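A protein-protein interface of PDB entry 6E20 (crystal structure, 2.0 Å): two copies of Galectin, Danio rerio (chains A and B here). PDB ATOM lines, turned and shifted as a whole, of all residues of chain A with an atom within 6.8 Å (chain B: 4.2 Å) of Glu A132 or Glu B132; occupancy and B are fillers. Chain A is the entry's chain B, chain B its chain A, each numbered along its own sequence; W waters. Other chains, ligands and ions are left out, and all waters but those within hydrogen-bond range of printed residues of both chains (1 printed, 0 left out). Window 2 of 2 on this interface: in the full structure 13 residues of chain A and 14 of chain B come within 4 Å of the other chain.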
ATOM      1  N   MET A   9      -2.643 -33.154   4.977  1.00  0.00           N
ATOM      2  CA  MET A   9      -2.126 -31.762   4.903  1.00  0.00           C
ATOM      3  C   MET A   9      -3.276 -30.851   4.439  1.00  0.00           C
ATOM      4  O   MET A   9      -3.446 -30.672   3.252  1.00  0.00           O
ATOM      5  CB  MET A   9      -0.939 -31.687   3.942  1.00  0.00           C
ATOM      6  CG  MET A   9      -0.100 -30.447   4.117  1.00  0.00           C
ATOM      7  SD  MET A   9       1.346 -30.433   3.036  1.00  0.00           S
ATOM      8  CE  MET A   9       1.970 -28.791   3.386  1.00  0.00           C
ATOM      9  N   PHE A  11      -5.940 -28.385   3.101  1.00  0.00           N
ATOM     10  CA  PHE A  11      -6.017 -27.214   2.193  1.00  0.00           C
ATOM     11  C   PHE A  11      -7.442 -26.660   2.267  1.00  0.00           C
ATOM     12  O   PHE A  11      -8.390 -27.329   1.790  1.00  0.00           O
ATOM     13  CB  PHE A  11      -5.648 -27.652   0.775  1.00  0.00           C
ATOM     14  CG  PHE A  11      -5.639 -26.571  -0.271  1.00  0.00           C
ATOM     15  CD1 PHE A  11      -5.222 -25.281   0.023  1.00  0.00           C
ATOM     16  CD2 PHE A  11      -6.002 -26.875  -1.580  1.00  0.00           C
ATOM     17  CE1 PHE A  11      -5.196 -24.306  -0.964  1.00  0.00           C
ATOM     18  CE2 PHE A  11      -5.981 -25.902  -2.565  1.00  0.00           C
ATOM     19  CZ  PHE A  11      -5.563 -24.625  -2.253  1.00  0.00           C
ATOM     20  N   THR A  16      -3.252 -20.307   0.163  1.00  0.00           N
ATOM     21  CA  THR A  16      -2.611 -20.596  -1.142  1.00  0.00           C
ATOM     22  C   THR A  16      -1.836 -21.900  -0.985  1.00  0.00           C
ATOM     23  O   THR A  16      -1.158 -22.092   0.049  1.00  0.00           O
ATOM     24  CB  THR A  16      -1.729 -19.445  -1.634  1.00  0.00           C
ATOM     25  OG1 THR A  16      -2.299 -18.222  -1.165  1.00  0.00           O
ATOM     26  CG2 THR A  16      -1.625 -19.405  -3.144  1.00  0.00           C
ATOM     27  N   LEU A  17      -1.990 -22.783  -1.960  1.00  0.00           N
ATOM     28  CA  LEU A  17      -1.148 -23.985  -2.133  1.00  0.00           C
ATOM     29  C   LEU A  17      -0.079 -23.667  -3.184  1.00  0.00           C
ATOM     30  O   LEU A  17      -0.464 -23.350  -4.316  1.00  0.00           O
ATOM     31  CB  LEU A  17      -2.054 -25.120  -2.580  1.00  0.00           C
ATOM     32  CG  LEU A  17      -1.343 -26.328  -3.174  1.00  0.00           C
ATOM     33  CD1 LEU A  17      -0.327 -26.897  -2.194  1.00  0.00           C
ATOM     34  CD2 LEU A  17      -2.371 -27.364  -3.578  1.00  0.00           C
ATOM     35  N   THR A  18       1.195 -23.724  -2.799  1.00  0.00           N
ATOM     36  CA  THR A  18       2.364 -23.494  -3.684  1.00  0.00           C
ATOM     37  C   THR A  18       2.995 -24.854  -3.970  1.00  0.00           C
ATOM     38  O   THR A  18       3.321 -25.549  -3.012  1.00  0.00           O
ATOM     39  CB  THR A  18       3.326 -22.460  -3.094  1.00  0.00           C
ATOM     40  OG1 THR A  18       2.571 -21.258  -2.879  1.00  0.00           O
ATOM     41  CG2 THR A  18       4.484 -22.146  -4.013  1.00  0.00           C
ATOM     42  N   ILE A  19       3.050 -25.240  -5.243  1.00  0.00           N
ATOM     43  CA  ILE A  19       3.636 -26.538  -5.697  1.00  0.00           C
ATOM     44  C   ILE A  19       4.878 -26.196  -6.496  1.00  0.00           C
ATOM     45  O   ILE A  19       4.749 -25.401  -7.458  1.00  0.00           O
ATOM     46  CB  ILE A  19       2.641 -27.372  -6.529  1.00  0.00           C
ATOM     47  CG1 ILE A  19       1.392 -27.731  -5.711  1.00  0.00           C
ATOM     48  CG2 ILE A  19       3.321 -28.625  -7.084  1.00  0.00           C
ATOM     49  CD1 ILE A  19       0.199 -28.132  -6.540  1.00  0.00           C
ATOM     50  N   THR A  20       6.019 -26.729  -6.067  1.00  0.00           N
ATOM     51  CA  THR A  20       7.315 -26.629  -6.784  1.00  0.00           C
ATOM     52  C   THR A  20       7.661 -28.012  -7.324  1.00  0.00           C
ATOM     53  O   THR A  20       7.648 -28.982  -6.555  1.00  0.00           O
ATOM     54  CB  THR A  20       8.442 -26.115  -5.886  1.00  0.00           C
ATOM     55  OG1 THR A  20       7.855 -25.074  -5.109  1.00  0.00           O
ATOM     56  CG2 THR A  20       9.622 -25.597  -6.677  1.00  0.00           C
ATOM     57  N   GLN A  86       6.799 -23.311 -10.521  1.00  0.00           N
ATOM     58  CA  GLN A  86       6.031 -23.005  -9.302  1.00  0.00           C
ATOM     59  C   GLN A  86       4.613 -22.622  -9.739  1.00  0.00           C
ATOM     60  O   GLN A  86       4.474 -21.791 -10.657  1.00  0.00           O
ATOM     61  CB  GLN A  86       6.747 -21.949  -8.460  1.00  0.00           C
ATOM     62  CG  GLN A  86       6.413 -22.105  -6.988  1.00  0.00           C
ATOM     63  CD  GLN A  86       7.211 -21.190  -6.090  1.00  0.00           C
ATOM     64  OE1 GLN A  86       6.879 -20.016  -5.933  1.00  0.00           O
ATOM     65  NE2 GLN A  86       8.219 -21.752  -5.442  1.00  0.00           N
ATOM     66  N   GLN A 129       9.050 -31.211  -5.599  1.00  0.00           N
ATOM     67  CA  GLN A 129      10.139 -30.722  -4.731  1.00  0.00           C
ATOM     68  C   GLN A 129       9.562 -29.892  -3.583  1.00  0.00           C
ATOM     69  O   GLN A 129      10.305 -29.710  -2.603  1.00  0.00           O
ATOM     70  CB  GLN A 129      11.109 -29.864  -5.541  1.00  0.00           C
ATOM     71  CG  GLN A 129      11.682 -30.584  -6.756  1.00  0.00           C
ATOM     72  CD  GLN A 129      12.680 -29.716  -7.491  1.00  0.00           C
ATOM     73  OE1 GLN A 129      12.459 -28.521  -7.730  1.00  0.00           O
ATOM     74  NE2 GLN A 129      13.797 -30.324  -7.865  1.00  0.00           N
ATOM     75  N   GLY A 130       8.343 -29.344  -3.723  1.00  0.00           N
ATOM     76  CA  GLY A 130       7.765 -28.474  -2.683  1.00  0.00           C
ATOM     77  C   GLY A 130       6.256 -28.477  -2.681  1.00  0.00           C
ATOM     78  O   GLY A 130       5.653 -28.366  -3.760  1.00  0.00           O
ATOM     79  N   VAL A 131       5.679 -28.648  -1.496  1.00  0.00           N
ATOM     80  CA  VAL A 131       4.240 -28.417  -1.208  1.00  0.00           C
ATOM     81  C   VAL A 131       4.182 -27.515   0.020  1.00  0.00           C
ATOM     82  O   VAL A 131       4.680 -27.938   1.094  1.00  0.00           O
ATOM     83  CB  VAL A 131       3.451 -29.717  -0.999  1.00  0.00           C
ATOM     84  CG1 VAL A 131       1.952 -29.445  -0.899  1.00  0.00           C
ATOM     85  CG2 VAL A 131       3.728 -30.688  -2.128  1.00  0.00           C
ATOM     86  N   GLU A 132       3.652 -26.312  -0.178  1.00  0.00           N
ATOM     87  CA  GLU A 132       3.473 -25.286   0.877  1.00  0.00           C
ATOM     88  C   GLU A 132       2.009 -24.854   0.885  1.00  0.00           C
ATOM     89  O   GLU A 132       1.473 -24.557  -0.204  1.00  0.00           O
ATOM     90  CB  GLU A 132       4.357 -24.070   0.614  1.00  0.00           C
ATOM     91  CG  GLU A 132       5.834 -24.395   0.603  1.00  0.00           C
ATOM     92  CD  GLU A 132       6.707 -23.293   0.027  1.00  0.00           C
ATOM     93  OE1 GLU A 132       6.721 -23.147  -1.207  1.00  0.00           O
ATOM     94  OE2 GLU A 132       7.359 -22.583   0.811  1.00  0.00           O
ATOM     95  N   ILE A 133       1.414 -24.779   2.072  1.00  0.00           N
ATOM     96  CA  ILE A 133       0.009 -24.324   2.277  1.00  0.00           C
ATOM     97  C   ILE A 133       0.030 -23.326   3.428  1.00  0.00           C
ATOM     98  O   ILE A 133       0.448 -23.741   4.517  1.00  0.00           O
ATOM     99  CB  ILE A 133      -0.936 -25.505   2.575  1.00  0.00           C
ATOM    100  CG1 ILE A 133      -0.986 -26.487   1.407  1.00  0.00           C
ATOM    101  CG2 ILE A 133      -2.330 -25.016   2.962  1.00  0.00           C
ATOM    102  CD1 ILE A 133      -1.695 -27.787   1.724  1.00  0.00           C
ATOM    103  N   LYS A 134      -0.395 -22.084   3.183  1.00  0.00           N
ATOM    104  CA  LYS A 134      -0.654 -21.072   4.246  1.00  0.00           C
ATOM    105  C   LYS A 134      -1.855 -20.217   3.835  1.00  0.00           C
ATOM    106  O   LYS A 134      -1.847 -19.645   2.766  1.00  0.00           O
ATOM    107  CB  LYS A 134       0.592 -20.212   4.487  1.00  0.00           C
ATOM    108  CG  LYS A 134       0.969 -19.313   3.320  1.00  0.00           C
ATOM    109  CD  LYS A 134       2.424 -18.929   3.300  1.00  0.00           C
ATOM    110  CE  LYS A 134       2.739 -17.903   2.228  1.00  0.00           C
ATOM    111  NZ  LYS A 134       4.139 -18.024   1.746  1.00  0.00           N
ATOM    112  OXT LYS A 134      -2.851 -20.089   4.537  1.00  0.00           O
ATOM    113  N   THR B  16      18.560 -30.073   0.922  1.00  0.00           N
ATOM    114  CA  THR B  16      17.938 -29.470   2.129  1.00  0.00           C
ATOM    115  C   THR B  16      16.451 -29.865   2.151  1.00  0.00           C
ATOM    116  O   THR B  16      15.730 -29.529   1.180  1.00  0.00           O
ATOM    117  CB  THR B  16      18.106 -27.940   2.137  1.00  0.00           C
ATOM    118  OG1 THR B  16      19.429 -27.575   1.745  1.00  0.00           O
ATOM    119  CG2 THR B  16      17.836 -27.316   3.488  1.00  0.00           C
ATOM    120  N   LEU B  17      16.006 -30.554   3.201  1.00  0.00           N
ATOM    121  CA  LEU B  17      14.563 -30.700   3.525  1.00  0.00           C
ATOM    122  C   LEU B  17      14.189 -29.544   4.448  1.00  0.00           C
ATOM    123  O   LEU B  17      14.830 -29.426   5.509  1.00  0.00           O
ATOM    124  CB  LEU B  17      14.295 -32.051   4.194  1.00  0.00           C
ATOM    125  CG  LEU B  17      12.872 -32.240   4.719  1.00  0.00           C
ATOM    126  CD1 LEU B  17      11.852 -32.170   3.587  1.00  0.00           C
ATOM    127  CD2 LEU B  17      12.735 -33.552   5.465  1.00  0.00           C
ATOM    128  N   THR B  18      13.259 -28.684   4.026  1.00  0.00           N
ATOM    129  CA  THR B  18      12.700 -27.587   4.858  1.00  0.00           C
ATOM    130  C   THR B  18      11.260 -27.952   5.272  1.00  0.00           C
ATOM    131  O   THR B  18      10.421 -28.162   4.378  1.00  0.00           O
ATOM    132  CB  THR B  18      12.784 -26.247   4.124  1.00  0.00           C
ATOM    133  OG1 THR B  18      14.148 -26.052   3.737  1.00  0.00           O
ATOM    134  CG2 THR B  18      12.292 -25.089   4.964  1.00  0.00           C
ATOM    135  N   GLN B 129       2.730 -26.845   7.368  1.00  0.00           N
ATOM    136  CA  GLN B 129       2.427 -25.836   6.325  1.00  0.00           C
ATOM    137  C   GLN B 129       3.393 -25.930   5.137  1.00  0.00           C
ATOM    138  O   GLN B 129       3.051 -25.360   4.079  1.00  0.00           O
ATOM    139  CB  GLN B 129       2.499 -24.431   6.914  1.00  0.00           C
ATOM    140  CG  GLN B 129       1.290 -24.106   7.779  1.00  0.00           C
ATOM    141  CD  GLN B 129       1.477 -22.881   8.640  1.00  0.00           C
ATOM    142  OE1 GLN B 129       2.590 -22.468   8.961  1.00  0.00           O
ATOM    143  NE2 GLN B 129       0.365 -22.306   9.051  1.00  0.00           N
ATOM    144  N   VAL B 131       6.610 -28.361   3.104  1.00  0.00           N
ATOM    145  CA  VAL B 131       7.564 -29.484   2.880  1.00  0.00           C
ATOM    146  C   VAL B 131       8.274 -29.271   1.539  1.00  0.00           C
ATOM    147  O   VAL B 131       7.604 -29.399   0.513  1.00  0.00           O
ATOM    148  CB  VAL B 131       6.852 -30.842   2.945  1.00  0.00           C
ATOM    149  CG1 VAL B 131       7.819 -31.993   2.727  1.00  0.00           C
ATOM    150  CG2 VAL B 131       6.092 -31.002   4.257  1.00  0.00           C
ATOM    151  N   GLU B 132       9.563 -28.905   1.568  1.00  0.00           N
ATOM    152  CA  GLU B 132      10.363 -28.648   0.340  1.00  0.00           C
ATOM    153  C   GLU B 132      11.758 -29.263   0.459  1.00  0.00           C
ATOM    154  O   GLU B 132      12.392 -29.133   1.534  1.00  0.00           O
ATOM    155  CB  GLU B 132      10.429 -27.164  -0.026  1.00  0.00           C
ATOM    156  CG  GLU B 132      10.672 -26.222   1.125  1.00  0.00           C
ATOM    157  CD  GLU B 132      10.042 -24.853   0.953  1.00  0.00           C
ATOM    158  OE1 GLU B 132      10.133 -24.271  -0.159  1.00  0.00           O
ATOM    159  OE2 GLU B 132       9.480 -24.360   1.937  1.00  0.00           O
ATOM    160  N   ILE B 133      12.210 -29.860  -0.651  1.00  0.00           N
ATOM    161  CA  ILE B 133      13.471 -30.649  -0.768  1.00  0.00           C
ATOM    162  C   ILE B 133      14.402 -29.965  -1.780  1.00  0.00           C
ATOM    163  O   ILE B 133      13.873 -29.598  -2.844  1.00  0.00           O
ATOM    164  CB  ILE B 133      13.147 -32.097  -1.167  1.00  0.00           C
ATOM    165  CG1 ILE B 133      12.236 -32.769  -0.143  1.00  0.00           C
ATOM    166  CG2 ILE B 133      14.427 -32.889  -1.376  1.00  0.00           C
ATOM    167  CD1 ILE B 133      11.817 -34.159  -0.531  1.00  0.00           C
HETATM  168  O   HOH W   1       9.807 -25.529  -2.781  1.00  0.00           O
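O of Gln B129 sits at hydrogen-bond distance from N of Ile A133 (2.7 Å).
N of Val B131 lies within hydrogen-bond range of O of Val A131, 2.8 Å away.
The backbone NH (N) of Ile B133 lies within hydrogen-bond range of the backbone carbonyl oxygen (O) of Gln A129, 2.7 Å away.
The side-chain carboxylate (OE2) of Glu A132 lies close to the side-chain carboxylate (OE2) of Glu B132, at 3.0 Å.
N of Thr B18 is in hydrogen-bond range of O of Glu B132 (2.7 Å).
The backbone NH (N) of Thr A18 is in hydrogen-bond range of the backbone carbonyl oxygen (O) of Glu A132 (2.7 Å).
O of Thr A20 sits at hydrogen-bond distance from N of Gln A129 (2.8 Å).
O of Gly A130 sits at hydrogen-bond distance from N of Thr A20 (2.9 Å).
Among the printed residues, merely in contact across the chains: Met A9 with Gln B129, Gln A129 with Glu B132, Gly A130 with Val B131, Gly A130 with Glu B132 and Glu A132 with Gln B129.
Thr A18 touches none of the printed residues of chain B.
Of the printed residues of chain B, Gln A129 touches Glu B132 and Ile B133.
Printed residues of chain B within 4 Å of Val A131: Val B131 (2.8 Å).
Printed residues of chain B within 4 Å of Glu A132: Gln B129 (3.2 Å) and Glu B132 (3.0 Å).
Of the printed residues of chain B, Ile A133 touches Gln B129 (2.7 Å).
Printed residues of chain A within 4 Å of Val B131: Gly A130 and Val A131.
Of the printed residues of chain A, Glu B132 touches Gln A129 (3.1 Å), Gly A130 (3.98 Å) and Glu A132 (3.0 Å).
The nearest printed residue of chain A that does not touch Glu B132 is Val A131 (5.0 Å).
The nearest printed residue of chain B that does not touch Gln A129 is Val B131 (4.1 Å).
Of the 14 printed residues of chain A, 6 touch a printed residue of chain B.
Hydrophobic or aromatic side chains of chain A within 4 Å of the printed part of chain B: Met A9.
Of the 7 printed residues of chain B, 4 touch a printed residue of chain A.
Hydrophobic or aromatic side chains of chain B within 4 Å of the printed part of chain A: Ile B133.
Gln A129 touches Glu B132, and with the chains exchanged Glu A132 touches Gln B129.
Gln A129 touches Ile B133, and with the chains exchanged Ile A133 touches Gln B129.
Val A131 touches its own counterpart, Val B131.
Glu A132 touches its own counterpart, Glu B132.
Positions printed for both chains: 16, 17, 18, 129, 131, 132 and 133.
Water W1 bridges OE1 of Glu B132 and OG1 of Thr A20.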
